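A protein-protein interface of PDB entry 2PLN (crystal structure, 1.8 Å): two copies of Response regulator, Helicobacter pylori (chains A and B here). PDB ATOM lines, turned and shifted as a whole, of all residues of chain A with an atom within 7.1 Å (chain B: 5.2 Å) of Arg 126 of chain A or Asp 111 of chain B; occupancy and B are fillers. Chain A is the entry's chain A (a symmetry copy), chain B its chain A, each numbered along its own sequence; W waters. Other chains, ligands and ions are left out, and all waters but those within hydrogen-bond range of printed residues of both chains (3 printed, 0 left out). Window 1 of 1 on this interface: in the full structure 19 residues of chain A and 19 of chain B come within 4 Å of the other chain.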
ATOM      1  N   LEU A  65      17.154  -3.879 -11.893  1.00  0.00           N
ATOM      2  CA  LEU A  65      17.932  -5.118 -11.645  1.00  0.00           C
ATOM      3  C   LEU A  65      17.879  -6.028 -12.865  1.00  0.00           C
ATOM      4  O   LEU A  65      16.851  -6.086 -13.563  1.00  0.00           O
ATOM      5  CB  LEU A  65      17.340  -5.850 -10.435  1.00  0.00           C
ATOM      6  CG  LEU A  65      18.128  -7.079  -9.931  1.00  0.00           C
ATOM      7  CD1 LEU A  65      18.030  -7.265  -8.421  1.00  0.00           C
ATOM      8  CD2 LEU A  65      17.672  -8.369 -10.665  1.00  0.00           C
ATOM      9  N   MET A  67      18.961 -10.110 -13.914  1.00  0.00           N
ATOM     10  CA  MET A  67      19.543 -11.398 -13.600  1.00  0.00           C
ATOM     11  C   MET A  67      19.853 -12.133 -14.891  1.00  0.00           C
ATOM     12  O   MET A  67      18.991 -12.270 -15.764  1.00  0.00           O
ATOM     13  CB  MET A  67      18.621 -12.249 -12.726  1.00  0.00           C
ATOM     14  CG  MET A  67      19.362 -13.486 -12.221  1.00  0.00           C
ATOM     15  SD  MET A  67      18.495 -14.395 -10.763  1.00  0.00           S
ATOM     16  CE  MET A  67      16.768 -14.679 -11.568  1.00  0.00           C
ATOM     17  N   LEU A  90      22.778  -9.604 -11.104  1.00  0.00           N
ATOM     18  CA  LEU A  90      22.848 -10.945 -10.471  1.00  0.00           C
ATOM     19  C   LEU A  90      23.201 -11.935 -11.549  1.00  0.00           C
ATOM     20  O   LEU A  90      22.586 -11.939 -12.624  1.00  0.00           O
ATOM     21  CB  LEU A  90      21.507 -11.356  -9.838  1.00  0.00           C
ATOM     22  CG  LEU A  90      20.729 -10.319  -9.002  1.00  0.00           C
ATOM     23  CD1 LEU A  90      19.532 -10.968  -8.292  1.00  0.00           C
ATOM     24  CD2 LEU A  90      21.666  -9.606  -7.958  1.00  0.00           C
ATOM     25  N   PHE A 105      32.106 -11.737  -9.017  1.00  0.00           N
ATOM     26  CA  PHE A 105      32.188 -10.703  -7.990  1.00  0.00           C
ATOM     27  C   PHE A 105      33.262  -9.666  -8.300  1.00  0.00           C
ATOM     28  O   PHE A 105      33.040  -8.452  -8.139  1.00  0.00           O
ATOM     29  CB  PHE A 105      32.406 -11.335  -6.636  1.00  0.00           C
ATOM     30  CG  PHE A 105      31.151 -11.877  -6.023  1.00  0.00           C
ATOM     31  CD1 PHE A 105      30.043 -11.012  -5.758  1.00  0.00           C
ATOM     32  CD2 PHE A 105      31.069 -13.204  -5.649  1.00  0.00           C
ATOM     33  CE1 PHE A 105      28.860 -11.508  -5.168  1.00  0.00           C
ATOM     34  CE2 PHE A 105      29.884 -13.722  -5.048  1.00  0.00           C
ATOM     35  CZ  PHE A 105      28.791 -12.864  -4.798  1.00  0.00           C
ATOM     36  N   ASP A 110      26.567  -8.209  -8.217  1.00  0.00           N
ATOM     37  CA  ASP A 110      26.047  -8.034  -6.878  1.00  0.00           C
ATOM     38  C   ASP A 110      25.729  -9.376  -6.238  1.00  0.00           C
ATOM     39  O   ASP A 110      25.624  -9.474  -5.005  1.00  0.00           O
ATOM     40  CB  ASP A 110      24.809  -7.139  -6.937  1.00  0.00           C
ATOM     41  CG  ASP A 110      25.151  -5.748  -7.380  1.00  0.00           C
ATOM     42  OD1 ASP A 110      25.799  -5.041  -6.575  1.00  0.00           O
ATOM     43  OD2 ASP A 110      24.865  -5.302  -8.504  1.00  0.00           O
ATOM     44  N   ASP A 111      25.565 -10.413  -7.063  1.00  0.00           N
ATOM     45  CA  ASP A 111      25.390 -11.724  -6.507  1.00  0.00           C
ATOM     46  C   ASP A 111      25.746 -12.778  -7.536  1.00  0.00           C
ATOM     47  O   ASP A 111      25.842 -12.500  -8.749  1.00  0.00           O
ATOM     48  CB  ASP A 111      23.931 -11.887  -6.036  1.00  0.00           C
ATOM     49  CG  ASP A 111      23.798 -12.775  -4.793  1.00  0.00           C
ATOM     50  OD1 ASP A 111      24.669 -13.668  -4.563  1.00  0.00           O
ATOM     51  OD2 ASP A 111      22.826 -12.650  -4.017  1.00  0.00           O
ATOM     52  N   TYR A 112      25.956 -13.987  -7.038  1.00  0.00           N
ATOM     53  CA  TYR A 112      26.216 -15.162  -7.855  1.00  0.00           C
ATOM     54  C   TYR A 112      25.371 -16.299  -7.280  1.00  0.00           C
ATOM     55  O   TYR A 112      25.486 -16.640  -6.088  1.00  0.00           O
ATOM     56  CB  TYR A 112      27.708 -15.499  -7.809  1.00  0.00           C
ATOM     57  CG  TYR A 112      28.112 -16.666  -8.689  1.00  0.00           C
ATOM     58  CD1 TYR A 112      28.314 -17.924  -8.141  1.00  0.00           C
ATOM     59  CD2 TYR A 112      28.307 -16.512 -10.081  1.00  0.00           C
ATOM     60  CE1 TYR A 112      28.711 -19.021  -8.957  1.00  0.00           C
ATOM     61  CE2 TYR A 112      28.707 -17.607 -10.889  1.00  0.00           C
ATOM     62  CZ  TYR A 112      28.892 -18.845 -10.319  1.00  0.00           C
ATOM     63  OH  TYR A 112      29.268 -19.945 -11.132  1.00  0.00           O
ATOM     64  N   ILE A 113      24.511 -16.880  -8.114  1.00  0.00           N
ATOM     65  CA  ILE A 113      23.471 -17.756  -7.590  1.00  0.00           C
ATOM     66  C   ILE A 113      23.562 -19.057  -8.382  1.00  0.00           C
ATOM     67  O   ILE A 113      23.532 -19.037  -9.601  1.00  0.00           O
ATOM     68  CB  ILE A 113      22.073 -17.091  -7.761  1.00  0.00           C
ATOM     69  CG1 ILE A 113      22.008 -15.745  -7.016  1.00  0.00           C
ATOM     70  CG2 ILE A 113      20.909 -18.047  -7.340  1.00  0.00           C
ATOM     71  CD1 ILE A 113      20.915 -14.863  -7.520  1.00  0.00           C
ATOM     72  N   ARG A 118      16.818 -22.533  -4.964  1.00  0.00           N
ATOM     73  CA  ARG A 118      16.262 -23.166  -3.757  1.00  0.00           C
ATOM     74  C   ARG A 118      14.742 -23.276  -3.873  1.00  0.00           C
ATOM     75  O   ARG A 118      14.134 -24.302  -3.517  1.00  0.00           O
ATOM     76  CB  ARG A 118      16.662 -22.393  -2.489  1.00  0.00           C
ATOM     77  CG  ARG A 118      16.599 -23.229  -1.214  1.00  0.00           C
ATOM     78  CD  ARG A 118      17.566 -22.813  -0.109  1.00  0.00           C
ATOM     79  NE  ARG A 118      18.932 -23.298  -0.337  1.00  0.00           N
ATOM     80  CZ  ARG A 118      19.930 -22.548  -0.803  1.00  0.00           C
ATOM     81  NH1 ARG A 118      19.727 -21.270  -1.089  1.00  0.00           N
ATOM     82  NH2 ARG A 118      21.142 -23.063  -0.981  1.00  0.00           N
ATOM     83  N   ILE A 120      11.380 -20.565  -5.943  1.00  0.00           N
ATOM     84  CA  ILE A 120      10.997 -19.229  -6.446  1.00  0.00           C
ATOM     85  C   ILE A 120      10.879 -18.206  -5.300  1.00  0.00           C
ATOM     86  O   ILE A 120      11.411 -17.096  -5.422  1.00  0.00           O
ATOM     87  CB  ILE A 120       9.706 -19.301  -7.304  1.00  0.00           C
ATOM     88  CG1 ILE A 120       9.944 -20.131  -8.570  1.00  0.00           C
ATOM     89  CG2 ILE A 120       9.129 -17.882  -7.540  1.00  0.00           C
ATOM     90  CD1 ILE A 120      10.936 -19.589  -9.573  1.00  0.00           C
ATOM     91  N   LYS A 121      10.237 -18.578  -4.175  1.00  0.00           N
ATOM     92  CA  LYS A 121      10.065 -17.655  -3.052  1.00  0.00           C
ATOM     93  C   LYS A 121      11.416 -17.184  -2.449  1.00  0.00           C
ATOM     94  O   LYS A 121      11.572 -16.019  -2.125  1.00  0.00           O
ATOM     95  CB  LYS A 121       9.163 -18.258  -1.943  1.00  0.00           C
ATOM     96  CG  LYS A 121       7.652 -18.090  -2.203  1.00  0.00           C
ATOM     97  CD  LYS A 121       6.823 -18.598  -1.005  1.00  0.00           C
ATOM     98  CE  LYS A 121       5.396 -18.928  -1.470  1.00  0.00           C
ATOM     99  NZ  LYS A 121       4.557 -19.475  -0.351  1.00  0.00           N
ATOM    100  N   ALA A 122      12.358 -18.105  -2.301  1.00  0.00           N
ATOM    101  CA  ALA A 122      13.706 -17.786  -1.812  1.00  0.00           C
ATOM    102  C   ALA A 122      14.454 -16.901  -2.826  1.00  0.00           C
ATOM    103  O   ALA A 122      15.167 -15.972  -2.428  1.00  0.00           O
ATOM    104  CB  ALA A 122      14.486 -19.068  -1.549  1.00  0.00           C
ATOM    105  N   LEU A 123      14.345 -17.218  -4.115  1.00  0.00           N
ATOM    106  CA  LEU A 123      14.968 -16.380  -5.148  1.00  0.00           C
ATOM    107  C   LEU A 123      14.385 -14.953  -5.130  1.00  0.00           C
ATOM    108  O   LEU A 123      15.119 -13.965  -5.186  1.00  0.00           O
ATOM    109  CB  LEU A 123      14.787 -17.021  -6.531  1.00  0.00           C
ATOM    110  CG  LEU A 123      15.240 -16.161  -7.713  1.00  0.00           C
ATOM    111  CD1 LEU A 123      16.726 -15.702  -7.537  1.00  0.00           C
ATOM    112  CD2 LEU A 123      15.023 -16.985  -8.986  1.00  0.00           C
ATOM    113  N   VAL A 124      13.059 -14.856  -5.031  1.00  0.00           N
ATOM    114  CA  VAL A 124      12.387 -13.562  -4.945  1.00  0.00           C
ATOM    115  C   VAL A 124      12.782 -12.749  -3.710  1.00  0.00           C
ATOM    116  O   VAL A 124      12.992 -11.525  -3.796  1.00  0.00           O
ATOM    117  CB  VAL A 124      10.842 -13.722  -5.095  1.00  0.00           C
ATOM    118  CG1 VAL A 124      10.121 -12.444  -4.749  1.00  0.00           C
ATOM    119  CG2 VAL A 124      10.505 -14.240  -6.531  1.00  0.00           C
ATOM    120  N   ALA A 125      12.876 -13.416  -2.562  1.00  0.00           N
ATOM    121  CA  ALA A 125      13.326 -12.776  -1.336  1.00  0.00           C
ATOM    122  C   ALA A 125      14.759 -12.198  -1.508  1.00  0.00           C
ATOM    123  O   ALA A 125      15.071 -11.103  -1.029  1.00  0.00           O
ATOM    124  CB  ALA A 125      13.281 -13.779  -0.180  1.00  0.00           C
ATOM    125  N   ARG A 126      15.614 -12.942  -2.192  1.00  0.00           N
ATOM    126  CA  ARG A 126      16.998 -12.490  -2.452  1.00  0.00           C
ATOM    127  C   ARG A 126      16.972 -11.251  -3.368  1.00  0.00           C
ATOM    128  O   ARG A 126      17.674 -10.288  -3.113  1.00  0.00           O
ATOM    129  CB  ARG A 126      17.802 -13.600  -3.124  1.00  0.00           C
ATOM    130  CG  ARG A 126      19.272 -13.241  -3.553  1.00  0.00           C
ATOM    131  CD  ARG A 126      20.041 -14.443  -4.055  1.00  0.00           C
ATOM    132  NE  ARG A 126      20.156 -15.453  -3.000  1.00  0.00           N
ATOM    133  CZ  ARG A 126      21.155 -15.513  -2.107  1.00  0.00           C
ATOM    134  NH1 ARG A 126      22.171 -14.646  -2.188  1.00  0.00           N
ATOM    135  NH2 ARG A 126      21.134 -16.451  -1.132  1.00  0.00           N
ATOM    136  N   ILE A 127      16.175 -11.315  -4.440  1.00  0.00           N
ATOM    137  CA  ILE A 127      16.058 -10.180  -5.373  1.00  0.00           C
ATOM    138  C   ILE A 127      15.531  -8.963  -4.644  1.00  0.00           C
ATOM    139  O   ILE A 127      16.077  -7.870  -4.800  1.00  0.00           O
ATOM    140  CB  ILE A 127      15.189 -10.552  -6.590  1.00  0.00           C
ATOM    141  CG1 ILE A 127      15.916 -11.617  -7.403  1.00  0.00           C
ATOM    142  CG2 ILE A 127      14.899  -9.322  -7.475  1.00  0.00           C
ATOM    143  CD1 ILE A 127      15.062 -12.255  -8.512  1.00  0.00           C
ATOM    144  N   GLU A 128      14.493  -9.166  -3.832  1.00  0.00           N
ATOM    145  CA  GLU A 128      13.988  -8.116  -2.951  1.00  0.00           C
ATOM    146  C   GLU A 128      15.083  -7.461  -2.122  1.00  0.00           C
ATOM    147  O   GLU A 128      15.173  -6.233  -2.074  1.00  0.00           O
ATOM    148  CB  GLU A 128      12.975  -8.686  -1.971  1.00  0.00           C
ATOM    149  CG  GLU A 128      11.562  -8.611  -2.431  1.00  0.00           C
ATOM    150  CD  GLU A 128      10.632  -8.989  -1.300  1.00  0.00           C
ATOM    151  OE1 GLU A 128       9.588  -8.370  -1.210  1.00  0.00           O
ATOM    152  OE2 GLU A 128      10.974  -9.873  -0.479  1.00  0.00           O
ATOM    153  N   ALA A 129      15.896  -8.295  -1.463  1.00  0.00           N
ATOM    154  CA  ALA A 129      16.999  -7.815  -0.627  1.00  0.00           C
ATOM    155  C   ALA A 129      18.040  -7.047  -1.448  1.00  0.00           C
ATOM    156  O   ALA A 129      18.589  -6.054  -0.991  1.00  0.00           O
ATOM    157  CB  ALA A 129      17.682  -8.981   0.116  1.00  0.00           C
ATOM    158  N   ARG A 130      18.311  -7.518  -2.662  1.00  0.00           N
ATOM    159  CA  ARG A 130      19.300  -6.861  -3.492  1.00  0.00           C
ATOM    160  C   ARG A 130      18.841  -5.500  -3.988  1.00  0.00           C
ATOM    161  O   ARG A 130      19.656  -4.698  -4.458  1.00  0.00           O
ATOM    162  CB  ARG A 130      19.646  -7.749  -4.659  1.00  0.00           C
ATOM    163  CG  ARG A 130      20.425  -8.967  -4.233  1.00  0.00           C
ATOM    164  CD  ARG A 130      21.925  -8.723  -3.908  1.00  0.00           C
ATOM    165  NE  ARG A 130      22.326  -9.903  -3.156  1.00  0.00           N
ATOM    166  CZ  ARG A 130      22.392  -9.973  -1.832  1.00  0.00           C
ATOM    167  NH1 ARG A 130      22.223  -8.875  -1.097  1.00  0.00           N
ATOM    168  NH2 ARG A 130      22.698 -11.138  -1.253  1.00  0.00           N
ATOM    169  N   LEU A 131      17.548  -5.230  -3.865  1.00  0.00           N
ATOM    170  CA  LEU A 131      17.000  -3.934  -4.273  1.00  0.00           C
ATOM    171  C   LEU A 131      16.650  -3.080  -3.073  1.00  0.00           C
ATOM    172  O   LEU A 131      16.117  -1.980  -3.219  1.00  0.00           O
ATOM    173  CB  LEU A 131      15.784  -4.132  -5.179  1.00  0.00           C
ATOM    174  CG  LEU A 131      16.139  -4.490  -6.628  1.00  0.00           C
ATOM    175  CD1 LEU A 131      14.901  -4.820  -7.387  1.00  0.00           C
ATOM    176  CD2 LEU A 131      16.853  -3.320  -7.296  1.00  0.00           C
ATOM    177  N   ARG A 132      16.982  -3.560  -1.886  1.00  0.00           N
ATOM    178  CA  ARG A 132      16.583  -2.859  -0.679  1.00  0.00           C
ATOM    179  C   ARG A 132      17.419  -1.603  -0.443  1.00  0.00           C
ATOM    180  O   ARG A 132      18.602  -1.559  -0.759  1.00  0.00           O
ATOM    181  CB  ARG A 132      16.612  -3.792   0.523  1.00  0.00           C
ATOM    182  CG  ARG A 132      15.509  -3.493   1.486  1.00  0.00           C
ATOM    183  CD  ARG A 132      15.498  -4.334   2.758  1.00  0.00           C
ATOM    184  NE  ARG A 132      15.159  -5.745   2.530  1.00  0.00           N
ATOM    185  CZ  ARG A 132      14.027  -6.177   1.980  1.00  0.00           C
ATOM    186  NH1 ARG A 132      13.091  -5.314   1.564  1.00  0.00           N
ATOM    187  NH2 ARG A 132      13.836  -7.475   1.837  1.00  0.00           N
ATOM    188  N   VAL B  89      25.245  -8.146   7.620  1.00  0.00           N
ATOM    189  CA  VAL B  89      24.988  -9.413   8.268  1.00  0.00           C
ATOM    190  C   VAL B  89      24.786 -10.525   7.234  1.00  0.00           C
ATOM    191  O   VAL B  89      23.900 -10.433   6.361  1.00  0.00           O
ATOM    192  CB  VAL B  89      23.739  -9.316   9.178  1.00  0.00           C
ATOM    193  CG1 VAL B  89      23.421 -10.668   9.770  1.00  0.00           C
ATOM    194  CG2 VAL B  89      23.924  -8.209  10.257  1.00  0.00           C
ATOM    195  N   LEU B  90      25.604 -11.564   7.337  1.00  0.00           N
ATOM    196  CA  LEU B  90      25.528 -12.743   6.436  1.00  0.00           C
ATOM    197  C   LEU B  90      25.169 -13.935   7.283  1.00  0.00           C
ATOM    198  O   LEU B  90      25.785 -14.167   8.334  1.00  0.00           O
ATOM    199  CB  LEU B  90      26.868 -13.018   5.730  1.00  0.00           C
ATOM    200  CG  LEU B  90      27.650 -11.832   5.130  1.00  0.00           C
ATOM    201  CD1 LEU B  90      28.845 -12.323   4.299  1.00  0.00           C
ATOM    202  CD2 LEU B  90      26.717 -10.912   4.259  1.00  0.00           C
ATOM    203  N   VAL B  91      24.152 -14.665   6.857  1.00  0.00           N
ATOM    204  CA  VAL B  91      23.714 -15.869   7.569  1.00  0.00           C
ATOM    205  C   VAL B  91      24.220 -17.019   6.733  1.00  0.00           C
ATOM    206  O   VAL B  91      24.001 -17.059   5.527  1.00  0.00           O
ATOM    207  CB  VAL B  91      22.156 -15.936   7.651  1.00  0.00           C
ATOM    208  CG1 VAL B  91      21.684 -17.289   8.143  1.00  0.00           C
ATOM    209  CG2 VAL B  91      21.619 -14.828   8.567  1.00  0.00           C
ATOM    210  N   GLU B 101      15.807 -19.305   4.340  1.00  0.00           N
ATOM    211  CA  GLU B 101      16.332 -18.257   3.427  1.00  0.00           C
ATOM    212  C   GLU B 101      15.392 -17.053   3.333  1.00  0.00           C
ATOM    213  O   GLU B 101      15.812 -15.881   3.496  1.00  0.00           O
ATOM    214  CB  GLU B 101      16.616 -18.849   2.056  1.00  0.00           C
ATOM    215  CG  GLU B 101      17.229 -17.850   1.082  1.00  0.00           C
ATOM    216  CD  GLU B 101      17.966 -18.500  -0.055  1.00  0.00           C
ATOM    217  OE1 GLU B 101      17.831 -19.713  -0.260  1.00  0.00           O
ATOM    218  OE2 GLU B 101      18.690 -17.791  -0.760  1.00  0.00           O
ATOM    219  N   PHE B 105      16.267 -13.172   4.853  1.00  0.00           N
ATOM    220  CA  PHE B 105      16.190 -11.945   4.066  1.00  0.00           C
ATOM    221  C   PHE B 105      15.120 -10.991   4.587  1.00  0.00           C
ATOM    222  O   PHE B 105      15.348  -9.772   4.684  1.00  0.00           O
ATOM    223  CB  PHE B 105      15.969 -12.278   2.609  1.00  0.00           C
ATOM    224  CG  PHE B 105      17.223 -12.685   1.896  1.00  0.00           C
ATOM    225  CD1 PHE B 105      18.335 -11.789   1.818  1.00  0.00           C
ATOM    226  CD2 PHE B 105      17.299 -13.904   1.252  1.00  0.00           C
ATOM    227  CE1 PHE B 105      19.516 -12.155   1.136  1.00  0.00           C
ATOM    228  CE2 PHE B 105      18.482 -14.290   0.555  1.00  0.00           C
ATOM    229  CZ  PHE B 105      19.579 -13.403   0.491  1.00  0.00           C
ATOM    230  N   ALA B 109      18.773  -9.783   6.733  1.00  0.00           N
ATOM    231  CA  ALA B 109      20.121 -10.306   6.383  1.00  0.00           C
ATOM    232  C   ALA B 109      20.533  -9.829   4.993  1.00  0.00           C
ATOM    233  O   ALA B 109      19.715  -9.694   4.115  1.00  0.00           O
ATOM    234  CB  ALA B 109      20.149 -11.841   6.451  1.00  0.00           C
ATOM    235  N   ASP B 110      21.822  -9.579   4.808  1.00  0.00           N
ATOM    236  CA  ASP B 110      22.343  -9.130   3.535  1.00  0.00           C
ATOM    237  C   ASP B 110      22.656 -10.308   2.628  1.00  0.00           C
ATOM    238  O   ASP B 110      22.761 -10.146   1.401  1.00  0.00           O
ATOM    239  CB  ASP B 110      23.585  -8.271   3.779  1.00  0.00           C
ATOM    240  CG  ASP B 110      23.249  -7.003   4.504  1.00  0.00           C
ATOM    241  OD1 ASP B 110      22.605  -6.140   3.866  1.00  0.00           O
ATOM    242  OD2 ASP B 110      23.537  -6.804   5.696  1.00  0.00           O
ATOM    243  N   ASP B 111      22.815 -11.496   3.217  1.00  0.00           N
ATOM    244  CA  ASP B 111      22.984 -12.662   2.399  1.00  0.00           C
ATOM    245  C   ASP B 111      22.623 -13.907   3.184  1.00  0.00           C
ATOM    246  O   ASP B 111      22.528 -13.889   4.429  1.00  0.00           O
ATOM    247  CB  ASP B 111      24.443 -12.729   1.903  1.00  0.00           C
ATOM    248  CG  ASP B 111      24.573 -13.337   0.502  1.00  0.00           C
ATOM    249  OD1 ASP B 111      23.697 -14.159   0.090  1.00  0.00           O
ATOM    250  OD2 ASP B 111      25.546 -13.058  -0.231  1.00  0.00           O
ATOM    251  N   TYR B 112      22.408 -14.983   2.444  1.00  0.00           N
ATOM    252  CA  TYR B 112      22.142 -16.302   2.997  1.00  0.00           C
ATOM    253  C   TYR B 112      22.982 -17.297   2.195  1.00  0.00           C
ATOM    254  O   TYR B 112      22.867 -17.381   0.958  1.00  0.00           O
ATOM    255  CB  TYR B 112      20.649 -16.616   2.881  1.00  0.00           C
ATOM    256  CG  TYR B 112      20.239 -17.940   3.498  1.00  0.00           C
ATOM    257  CD1 TYR B 112      20.032 -19.055   2.698  1.00  0.00           C
ATOM    258  CD2 TYR B 112      20.044 -18.080   4.891  1.00  0.00           C
ATOM    259  CE1 TYR B 112      19.630 -20.297   3.267  1.00  0.00           C
ATOM    260  CE2 TYR B 112      19.639 -19.318   5.452  1.00  0.00           C
ATOM    261  CZ  TYR B 112      19.448 -20.409   4.635  1.00  0.00           C
ATOM    262  OH  TYR B 112      19.067 -21.653   5.200  1.00  0.00           O
ATOM    263  N   ILE B 113      23.840 -18.045   2.889  1.00  0.00           N
ATOM    264  CA  ILE B 113      24.876 -18.796   2.193  1.00  0.00           C
ATOM    265  C   ILE B 113      24.779 -20.233   2.694  1.00  0.00           C
ATOM    266  O   ILE B 113      24.809 -20.470   3.890  1.00  0.00           O
ATOM    267  CB  ILE B 113      26.277 -18.188   2.498  1.00  0.00           C
ATOM    268  CG1 ILE B 113      26.348 -16.716   2.052  1.00  0.00           C
ATOM    269  CG2 ILE B 113      27.437 -19.039   1.885  1.00  0.00           C
ATOM    270  CD1 ILE B 113      27.445 -15.964   2.729  1.00  0.00           C
ATOM    271  N   ARG B 126      32.757 -12.993  -2.080  1.00  0.00           N
ATOM    272  CA  ARG B 126      31.374 -12.598  -1.731  1.00  0.00           C
ATOM    273  C   ARG B 126      31.405 -11.579  -0.576  1.00  0.00           C
ATOM    274  O   ARG B 126      30.708 -10.581  -0.622  1.00  0.00           O
ATOM    275  CB  ARG B 126      30.565 -13.821  -1.306  1.00  0.00           C
ATOM    276  CG  ARG B 126      29.097 -13.553  -0.810  1.00  0.00           C
ATOM    277  CD  ARG B 126      28.322 -14.831  -0.571  1.00  0.00           C
ATOM    278  NE  ARG B 126      28.203 -15.597  -1.815  1.00  0.00           N
ATOM    279  CZ  ARG B 126      27.205 -15.464  -2.700  1.00  0.00           C
ATOM    280  NH1 ARG B 126      26.193 -14.628  -2.438  1.00  0.00           N
ATOM    281  NH2 ARG B 126      27.222 -16.177  -3.849  1.00  0.00           N
ATOM    282  N   ARG B 130      30.084  -7.775  -0.483  1.00  0.00           N
ATOM    283  CA  ARG B 130      29.097  -7.302   0.467  1.00  0.00           C
ATOM    284  C   ARG B 130      29.561  -6.077   1.237  1.00  0.00           C
ATOM    285  O   ARG B 130      28.750  -5.388   1.865  1.00  0.00           O
ATOM    286  CB  ARG B 130      28.747  -8.414   1.422  1.00  0.00           C
ATOM    287  CG  ARG B 130      27.963  -9.512   0.751  1.00  0.00           C
ATOM    288  CD  ARG B 130      26.464  -9.199   0.485  1.00  0.00           C
ATOM    289  NE  ARG B 130      26.058 -10.193  -0.498  1.00  0.00           N
ATOM    290  CZ  ARG B 130      25.992  -9.984  -1.807  1.00  0.00           C
ATOM    291  NH1 ARG B 130      26.167  -8.757  -2.295  1.00  0.00           N
ATOM    292  NH2 ARG B 130      25.681 -11.000  -2.617  1.00  0.00           N
HETATM  293  O   HOH W   1      17.609  -7.667   3.639  1.00  0.00           O
HETATM  294  O   HOH W   2      18.027 -17.302  -3.164  1.00  0.00           O
HETATM  295  O   HOH W   3      21.533 -20.227   0.615  1.00  0.00           O
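NH2 of Arg 126 of chain B is in hydrogen-bond range of O of Tyr 112 of chain A (2.9 Å). The side-chain carboxylate (OD1) of Asp 111 of chain A lies within salt-bridge range of the guanidinium group (NH1) of Arg 126 of chain B. The guanidinium group (NH2) of Arg 130 of chain B sits close to the guanidinium group (NH2) of Arg 130 of chain A (3.3 Å). OE1 of Glu 101 of chain B lies within salt-bridge range of NH1 of Arg 118 of chain A (2.6 Å). OD1 of Asp 111 of chain B is in salt-bridge range of NH2 of Arg 130 of chain A, 3.5 Å away. The guanidinium group (NH2) of Arg 126 of chain A is in salt-bridge range of the side-chain carboxylate (OE2) of Glu 101 of chain B (2.8 Å). The guanidinium group (NH2) of Arg 130 of chain B sits at hydrogen-bond distance from the backbone carbonyl oxygen (O) of Asp 110 of chain A, at 2.8 Å. OD1 of Asp 111 of chain B is in salt-bridge range of NH1 of Arg 126 of chain A (2.8 Å). The backbone carbonyl oxygen (O) of Asp 110 of chain B is in hydrogen-bond range of the guanidinium group (NH2) of Arg 130 of chain A, at 2.8 Å. The guanidinium group (NH2) of Arg 126 of chain A is in hydrogen-bond range of the backbone carbonyl oxygen (O) of Tyr 112 of chain B (2.9 Å). The guanidinium group of Arg 130 of chain B lies within salt-bridge range of the side-chain carboxylate of Asp 111 of chain A (3.5 Å).
O of Val 89 of chain B is in hydrogen-bond range of N of Asp 110 of chain B (2.7 Å). The side-chain carboxylate of Asp 111 of chain B lies within salt-bridge range of the guanidinium group of Arg 130 of chain B, 2.9 Å away. OD2 of Asp 111 of chain A lies within salt-bridge range of NE of Arg 130 of chain A (2.9 Å). O of Asp 111 of chain B sits at hydrogen-bond distance from N of Val 91 of chain B (3.0 Å). The guanidinium group of Arg 126 of chain A is in salt-bridge range of the side-chain carboxylate of Asp 111 of chain A.
Phe 105 of chain A touches Arg 126 of chain B (CZ to CZ, 3.7 Å). Ala 122 of chain A touches Glu 101 of chain B (CB to OE1, 3.6 Å). Ala 125 of chain A touches Phe 105 of chain B. CZ of Phe 105 of chain B touches CZ of Arg 126 of chain A, at 3.7 Å. CD1 of Phe 105 of chain B touches CB of Ala 129 of chain A, 3.3 Å away. Phe 105 of chain B touches Arg 132 of chain A (O to NH2, 3.96 Å).
Arg 126 of chain A touches four residues of chain B. Of chain A, only Arg 126 and Arg 130 come within 4 Å of Asp 111 of chain B. Printed residues of chain B within 4 Å of Asp 110 of chain A: Arg 130. Printed residues of chain A within 4 Å of Arg 130 of chain B: Asp 110, Asp 111 and Arg 130. The nearest residue of chain B that does not touch Arg 126 of chain A is Arg 126 of chain B (4.03 Å). The nearest printed residue of chain A that does not touch Tyr 112 of chain B is Arg 118 of chain A (4.4 Å).
Hydrophobic or aromatic side chains of chain A that line the printed part of chain B: Phe 105, Ala 122 and Ala 129. Of the 12 printed residues of chain B, 7 touch a printed residue of chain A. Hydrophobic or aromatic side chains of chain B within 4 Å of the printed part of chain A: Phe 105.
Phe 105 of chain A touches Arg 126 of chain B, and with the chains exchanged Arg 126 of chain A touches Phe 105 of chain B. Asp 110 of chain A touches Arg 130 of chain B, and with the chains exchanged Arg 130 of chain A touches Asp 110 of chain B. Tyr 112 of chain A touches Arg 126 of chain B, and with the chains exchanged Arg 126 of chain A touches Tyr 112 of chain B. Of the 17 pairs that touch across the chains among the printed residues, 11 have their exchanged pair printed and touching as well.
Water W2 lies within hydrogen-bond range of the side-chain carboxylate of Glu 101 of chain B (2.5 Å), the guanidinium group of Arg 126 of chain A (2.8 Å) and the backbone carbonyl oxygen of Ala 122 of chain A (3.2 Å). Water W3 bridges NH1 of Arg 118 of chain A and O of Tyr 112 of chain B. Water W1 lies within hydrogen-bond range of O of Ala 109 of chain B (3.0 Å), O of Phe 105 of chain B (3.3 Å) and NE of Arg 132 of chain A (3.3 Å).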
